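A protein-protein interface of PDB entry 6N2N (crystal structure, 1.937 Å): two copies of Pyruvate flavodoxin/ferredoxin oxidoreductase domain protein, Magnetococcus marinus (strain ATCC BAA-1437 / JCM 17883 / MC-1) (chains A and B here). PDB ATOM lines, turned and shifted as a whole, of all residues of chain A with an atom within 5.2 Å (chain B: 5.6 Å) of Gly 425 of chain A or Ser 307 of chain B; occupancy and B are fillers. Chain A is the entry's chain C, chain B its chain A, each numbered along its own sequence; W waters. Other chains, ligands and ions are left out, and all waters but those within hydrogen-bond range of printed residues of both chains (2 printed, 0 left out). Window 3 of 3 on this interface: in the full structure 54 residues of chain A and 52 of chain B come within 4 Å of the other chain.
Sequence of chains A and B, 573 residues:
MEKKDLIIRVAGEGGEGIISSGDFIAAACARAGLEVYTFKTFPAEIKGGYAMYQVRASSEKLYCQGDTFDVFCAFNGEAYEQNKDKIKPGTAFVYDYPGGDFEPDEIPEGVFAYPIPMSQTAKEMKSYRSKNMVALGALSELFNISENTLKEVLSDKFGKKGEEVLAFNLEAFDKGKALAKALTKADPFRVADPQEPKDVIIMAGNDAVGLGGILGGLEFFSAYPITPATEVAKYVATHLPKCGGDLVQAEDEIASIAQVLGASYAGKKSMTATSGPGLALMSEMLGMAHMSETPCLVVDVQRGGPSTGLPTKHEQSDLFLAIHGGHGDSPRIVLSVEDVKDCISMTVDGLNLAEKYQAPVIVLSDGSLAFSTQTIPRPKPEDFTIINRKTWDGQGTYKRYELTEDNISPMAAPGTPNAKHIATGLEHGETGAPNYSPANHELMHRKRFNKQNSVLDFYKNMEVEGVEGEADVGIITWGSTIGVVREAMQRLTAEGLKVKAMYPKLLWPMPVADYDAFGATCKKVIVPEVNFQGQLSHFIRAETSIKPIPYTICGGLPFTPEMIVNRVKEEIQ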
ATOM      1  N   GLU A 284      12.252   8.998 -18.086  1.00  0.00           N
ATOM      2  CA  GLU A 284      10.901   8.446 -18.008  1.00  0.00           C
ATOM      3  C   GLU A 284       9.849   9.527 -18.244  1.00  0.00           C
ATOM      4  O   GLU A 284       8.912   9.339 -19.029  1.00  0.00           O
ATOM      5  CB  GLU A 284      10.656   7.757 -16.658  1.00  0.00           C
ATOM      6  CG  GLU A 284       9.529   6.692 -16.758  1.00  0.00           C
ATOM      7  CD  GLU A 284       8.753   6.454 -15.466  1.00  0.00           C
ATOM      8  OE1 GLU A 284       9.057   7.096 -14.433  1.00  0.00           O
ATOM      9  OE2 GLU A 284       7.821   5.617 -15.495  1.00  0.00           O
ATOM     10  N   GLY A 287       9.339  10.555 -21.722  1.00  0.00           N
ATOM     11  CA  GLY A 287       8.452   9.635 -22.422  1.00  0.00           C
ATOM     12  C   GLY A 287       6.996  10.031 -22.277  1.00  0.00           C
ATOM     13  O   GLY A 287       6.232   9.982 -23.240  1.00  0.00           O
ATOM     14  N   MET A 288       6.596  10.432 -21.064  1.00  0.00           N
ATOM     15  CA  MET A 288       5.240  10.920 -20.827  1.00  0.00           C
ATOM     16  C   MET A 288       4.938  12.138 -21.689  1.00  0.00           C
ATOM     17  O   MET A 288       3.839  12.263 -22.247  1.00  0.00           O
ATOM     18  CB  MET A 288       5.071  11.261 -19.345  1.00  0.00           C
ATOM     19  CG  MET A 288       3.778  11.992 -18.978  1.00  0.00           C
ATOM     20  SD  MET A 288       2.339  10.917 -19.121  1.00  0.00           S
ATOM     21  CE  MET A 288       1.006  12.026 -18.641  1.00  0.00           C
ATOM     22  N   MET A 291       4.360  10.807 -25.319  1.00  0.00           N
ATOM     23  CA  MET A 291       3.145  10.011 -25.488  1.00  0.00           C
ATOM     24  C   MET A 291       1.890  10.846 -25.267  1.00  0.00           C
ATOM     25  O   MET A 291       0.911  10.713 -26.012  1.00  0.00           O
ATOM     26  CB  MET A 291       3.164   8.817 -24.535  1.00  0.00           C
ATOM     27  CG  MET A 291       1.838   8.052 -24.438  1.00  0.00           C
ATOM     28  SD  MET A 291       1.342   7.288 -25.995  1.00  0.00           S
ATOM     29  CE  MET A 291       1.838   5.580 -25.743  1.00  0.00           C
ATOM     30  N   SER A 292       1.887  11.697 -24.242  1.00  0.00           N
ATOM     31  CA  SER A 292       0.724  12.522 -23.936  1.00  0.00           C
ATOM     32  C   SER A 292       0.660  13.788 -24.779  1.00  0.00           C
ATOM     33  O   SER A 292      -0.328  14.522 -24.682  1.00  0.00           O
ATOM     34  CB  SER A 292       0.721  12.902 -22.454  1.00  0.00           C
ATOM     35  OG  SER A 292       1.715  13.877 -22.193  1.00  0.00           O
ATOM     36  N   HIS A 327      12.493   4.894 -23.256  1.00  0.00           N
ATOM     37  CA  HIS A 327      12.104   3.519 -23.530  1.00  0.00           C
ATOM     38  C   HIS A 327      11.015   3.496 -24.593  1.00  0.00           C
ATOM     39  O   HIS A 327      10.270   4.466 -24.770  1.00  0.00           O
ATOM     40  CB  HIS A 327      11.626   2.808 -22.257  1.00  0.00           C
ATOM     41  CG  HIS A 327      10.322   3.308 -21.716  1.00  0.00           C
ATOM     42  ND1 HIS A 327      10.229   4.421 -20.909  1.00  0.00           N
ATOM     43  CD2 HIS A 327       9.061   2.828 -21.842  1.00  0.00           C
ATOM     44  CE1 HIS A 327       8.966   4.616 -20.573  1.00  0.00           C
ATOM     45  NE2 HIS A 327       8.236   3.661 -21.123  1.00  0.00           N
ATOM     46  N   SER A 330      10.326   6.563 -28.707  1.00  0.00           N
ATOM     47  CA  SER A 330       9.991   7.725 -27.877  1.00  0.00           C
ATOM     48  C   SER A 330      10.832   8.923 -28.305  1.00  0.00           C
ATOM     49  O   SER A 330      11.749   9.348 -27.594  1.00  0.00           O
ATOM     50  CB  SER A 330      10.213   7.388 -26.400  1.00  0.00           C
ATOM     51  OG  SER A 330       9.541   8.280 -25.525  1.00  0.00           O
ATOM     52  N   ALA A 423      -5.375  13.744 -20.381  1.00  0.00           N
ATOM     53  CA  ALA A 423      -4.032  13.603 -20.919  1.00  0.00           C
ATOM     54  C   ALA A 423      -3.401  12.391 -20.248  1.00  0.00           C
ATOM     55  O   ALA A 423      -3.533  12.208 -19.035  1.00  0.00           O
ATOM     56  CB  ALA A 423      -3.200  14.865 -20.668  1.00  0.00           C
ATOM     57  N   THR A 424      -2.733  11.550 -21.033  1.00  0.00           N
ATOM     58  CA  THR A 424      -2.390  10.240 -20.504  1.00  0.00           C
ATOM     59  C   THR A 424      -1.081   9.738 -21.095  1.00  0.00           C
ATOM     60  O   THR A 424      -0.715  10.084 -22.222  1.00  0.00           O
ATOM     61  CB  THR A 424      -3.531   9.249 -20.791  1.00  0.00           C
ATOM     62  OG1 THR A 424      -3.223   7.964 -20.240  1.00  0.00           O
ATOM     63  CG2 THR A 424      -3.743   9.118 -22.281  1.00  0.00           C
ATOM     64  N   GLY A 425      -0.371   8.924 -20.304  1.00  0.00           N
ATOM     65  CA  GLY A 425       0.803   8.202 -20.757  1.00  0.00           C
ATOM     66  C   GLY A 425       0.545   6.805 -21.285  1.00  0.00           C
ATOM     67  O   GLY A 425       1.445   6.197 -21.867  1.00  0.00           O
ATOM     68  N   LEU A 426      -0.657   6.266 -21.080  1.00  0.00           N
ATOM     69  CA  LEU A 426      -1.039   5.019 -21.724  1.00  0.00           C
ATOM     70  C   LEU A 426      -1.292   5.259 -23.206  1.00  0.00           C
ATOM     71  O   LEU A 426      -1.695   6.352 -23.618  1.00  0.00           O
ATOM     72  CB  LEU A 426      -2.299   4.444 -21.073  1.00  0.00           C
ATOM     73  CG  LEU A 426      -2.188   3.718 -19.730  1.00  0.00           C
ATOM     74  CD1 LEU A 426      -3.575   3.555 -19.124  1.00  0.00           C
ATOM     75  CD2 LEU A 426      -1.544   2.341 -19.923  1.00  0.00           C
ATOM     76  N   GLU A 427      -1.031   4.240 -24.021  1.00  0.00           N
ATOM     77  CA  GLU A 427      -1.486   4.320 -25.400  1.00  0.00           C
ATOM     78  C   GLU A 427      -3.005   4.439 -25.400  1.00  0.00           C
ATOM     79  O   GLU A 427      -3.689   3.839 -24.569  1.00  0.00           O
ATOM     80  CB  GLU A 427      -1.036   3.112 -26.221  1.00  0.00           C
ATOM     81  CG  GLU A 427      -1.425   3.228 -27.702  1.00  0.00           C
ATOM     82  CD  GLU A 427      -0.772   4.429 -28.391  1.00  0.00           C
ATOM     83  OE1 GLU A 427       0.202   4.233 -29.142  1.00  0.00           O
ATOM     84  OE2 GLU A 427      -1.228   5.573 -28.189  1.00  0.00           O
ATOM     85  N   PRO B 277       9.880   1.393 -18.429  1.00  0.00           N
ATOM     86  CA  PRO B 277       9.875   2.538 -17.499  1.00  0.00           C
ATOM     87  C   PRO B 277      10.943   2.433 -16.425  1.00  0.00           C
ATOM     88  O   PRO B 277      11.603   3.433 -16.097  1.00  0.00           O
ATOM     89  CB  PRO B 277       8.461   2.493 -16.903  1.00  0.00           C
ATOM     90  CG  PRO B 277       7.634   1.811 -17.968  1.00  0.00           C
ATOM     91  CD  PRO B 277       8.535   0.795 -18.585  1.00  0.00           C
ATOM     92  N   ARG B 303       8.038  -4.320 -22.817  1.00  0.00           N
ATOM     93  CA  ARG B 303       6.595  -4.243 -22.990  1.00  0.00           C
ATOM     94  C   ARG B 303       6.287  -3.135 -23.994  1.00  0.00           C
ATOM     95  O   ARG B 303       7.189  -2.474 -24.523  1.00  0.00           O
ATOM     96  CB  ARG B 303       5.888  -3.981 -21.651  1.00  0.00           C
ATOM     97  CG  ARG B 303       6.066  -2.553 -21.129  1.00  0.00           C
ATOM     98  CD  ARG B 303       5.588  -2.404 -19.684  1.00  0.00           C
ATOM     99  NE  ARG B 303       5.066  -1.067 -19.408  1.00  0.00           N
ATOM    100  CZ  ARG B 303       4.521  -0.710 -18.248  1.00  0.00           C
ATOM    101  NH1 ARG B 303       4.453  -1.585 -17.256  1.00  0.00           N
ATOM    102  NH2 ARG B 303       4.028   0.511 -18.082  1.00  0.00           N
ATOM    103  N   GLY B 304       5.002  -2.922 -24.253  1.00  0.00           N
ATOM    104  CA  GLY B 304       4.605  -1.881 -25.187  1.00  0.00           C
ATOM    105  C   GLY B 304       4.922  -0.499 -24.639  1.00  0.00           C
ATOM    106  O   GLY B 304       4.572  -0.169 -23.499  1.00  0.00           O
ATOM    107  N   GLY B 305       5.615   0.301 -25.441  1.00  0.00           N
ATOM    108  CA  GLY B 305       5.841   1.693 -25.131  1.00  0.00           C
ATOM    109  C   GLY B 305       5.255   2.545 -26.236  1.00  0.00           C
ATOM    110  O   GLY B 305       4.566   2.034 -27.120  1.00  0.00           O
ATOM    111  N   PRO B 306       5.545   3.855 -26.242  1.00  0.00           N
ATOM    112  CA  PRO B 306       6.368   4.577 -25.258  1.00  0.00           C
ATOM    113  C   PRO B 306       5.594   4.901 -23.983  1.00  0.00           C
ATOM    114  O   PRO B 306       4.393   4.616 -23.912  1.00  0.00           O
ATOM    115  CB  PRO B 306       6.748   5.858 -26.000  1.00  0.00           C
ATOM    116  CG  PRO B 306       5.586   6.110 -26.907  1.00  0.00           C
ATOM    117  CD  PRO B 306       5.088   4.739 -27.332  1.00  0.00           C
ATOM    118  N   SER B 307       6.279   5.495 -23.005  1.00  0.00           N
ATOM    119  CA  SER B 307       5.678   5.889 -21.735  1.00  0.00           C
ATOM    120  C   SER B 307       4.983   4.698 -21.080  1.00  0.00           C
ATOM    121  O   SER B 307       5.502   3.576 -21.126  1.00  0.00           O
ATOM    122  CB  SER B 307       4.710   7.059 -21.952  1.00  0.00           C
ATOM    123  OG  SER B 307       4.369   7.703 -20.735  1.00  0.00           O
ATOM    124  N   THR B 308       3.833   4.922 -20.441  1.00  0.00           N
ATOM    125  CA  THR B 308       3.114   3.803 -19.836  1.00  0.00           C
ATOM    126  C   THR B 308       2.741   2.765 -20.893  1.00  0.00           C
ATOM    127  O   THR B 308       2.877   1.558 -20.664  1.00  0.00           O
ATOM    128  CB  THR B 308       1.884   4.312 -19.081  1.00  0.00           C
ATOM    129  OG1 THR B 308       2.271   5.406 -18.234  1.00  0.00           O
ATOM    130  CG2 THR B 308       1.315   3.225 -18.203  1.00  0.00           C
ATOM    131  N   GLY B 309       2.292   3.217 -22.061  1.00  0.00           N
ATOM    132  CA  GLY B 309       2.319   2.365 -23.243  1.00  0.00           C
ATOM    133  C   GLY B 309       1.259   1.282 -23.236  1.00  0.00           C
ATOM    134  O   GLY B 309       0.067   1.544 -23.028  1.00  0.00           O
HETATM  135  O   HOH W   1       6.868   7.551 -19.386  1.00  0.00           O
HETATM  136  O   HOH W   2       9.115   6.476 -23.457  1.00  0.00           O
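N of Thr 308 of chain B lies within hydrogen-bond range of O of Gly 425 of chain A. The backbone carbonyl oxygen (O) of Gly 309 of chain B sits at hydrogen-bond distance from the backbone NH (N) of Glu 427 of chain A (3.1 Å). The backbone carbonyl oxygen of Ser 307 of chain B lies within hydrogen-bond range of a ring nitrogen (NE2) of His 327 of chain A (2.7 Å). N of Gly 309 of chain B sits at hydrogen-bond distance from O of Gly 425 of chain A. The side-chain hydroxyl (OG) of Ser 307 of chain B lies close to the backbone carbonyl oxygen (O) of Gly 425 of chain A (3.5 Å).
The backbone NH of Leu 426 of chain A lies within hydrogen-bond range of the side-chain hydroxyl of Thr 424 of chain A. The guanidinium group (NH2) of Arg 303 of chain B sits at hydrogen-bond distance from the backbone carbonyl oxygen (O) of Thr 308 of chain B (3.0 Å). The side-chain hydroxyl (OG) of Ser 292 of chain A lies within hydrogen-bond range of the backbone carbonyl oxygen (O) of Met 288 of chain A (2.7 Å). SD of Met 288 of chain A sits close to N of Gly 425 of chain A (3.6 Å).
Glu 284 of chain A touches Pro 277 of chain B (OE2 to CB, 3.5 Å). O of Gly 287 of chain A touches CB of Ser 307 of chain B (3.5 Å). Ser 307 of chain B touches Met 288 of chain A (OG to CA, 3.3 Å). O of Pro 306 of chain B touches CE of Met 291 of chain A, at 3.3 Å. CG of Pro 277 of chain B touches NE2 of His 327 of chain A, 3.7 Å away. His 327 of chain A touches Pro 306 of chain B (O to CA, 3.9 Å). Pro 306 of chain B touches Ser 330 of chain A. O of Pro 306 of chain B touches O of Gly 425 of chain A (3.9 Å). Thr 308 of chain B touches Leu 426 of chain A. Leu 426 of chain A touches Gly 309 of chain B (CD2 to O, 3.6 Å).
Of chain A, only Gly 287 (3.5 Å), Met 288 (3.3 Å), Met 291 (3.5 Å), His 327 (2.7 Å) and Gly 425 (3.4 Å) come within 4 Å of Ser 307 of chain B. Of the printed residues of chain B, Met 288 of chain A touches Ser 307 (3.3 Å). Of the printed residues of chain B, Gly 287 of chain A touches Ser 307. Printed residues of chain A within 4 Å of Pro 277 of chain B: Glu 284 and His 327. The nearest printed residue of chain B that does not touch Gly 425 of chain A is Gly 305 of chain B (6.9 Å). The nearest printed residue of chain B that does not touch His 327 of chain A is Thr 308 of chain B (4.6 Å).
Of the 12 printed residues of chain A, 9 touch a printed residue of chain B. Hydrophobic or aromatic side chains of chain A that line the printed part of chain B: Met 288, Met 291, His 327 and Leu 426. Along chain A the printed residues that touch a printed residue of chain B span positions 284 to 427. Printed residues of chain B that touch a printed residue of chain A: Pro 277, Pro 306, Ser 307, Thr 308 and Gly 309. Hydrophobic or aromatic side chains of chain B within 4 Å of the printed part of chain A: Pro 277 and Pro 306. Among the printed residues, 16 pairs touch across the chains. Among the printed residues, no Asp or Glu carboxylate lies within 4 Å of a Lys or Arg side-chain nitrogen of the other chain.
No position is printed for both chains. Of the 16 pairs that touch across the chains among the printed residues, none has its exchanged pair printed and touching as well.
Water W2 lies within hydrogen-bond range of the backbone carbonyl oxygen of His 327 of chain A (2.7 Å), the side-chain hydroxyl of Ser 330 of chain A (2.8 Å) and the backbone NH of Ser 307 of chain B (3.0 Å). Water W1 lies within hydrogen-bond range of O of Glu 284 of chain A (2.7 Å), OG of Ser 307 of chain B (2.8 Å) and N of Met 288 of chain A (3.3 Å).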
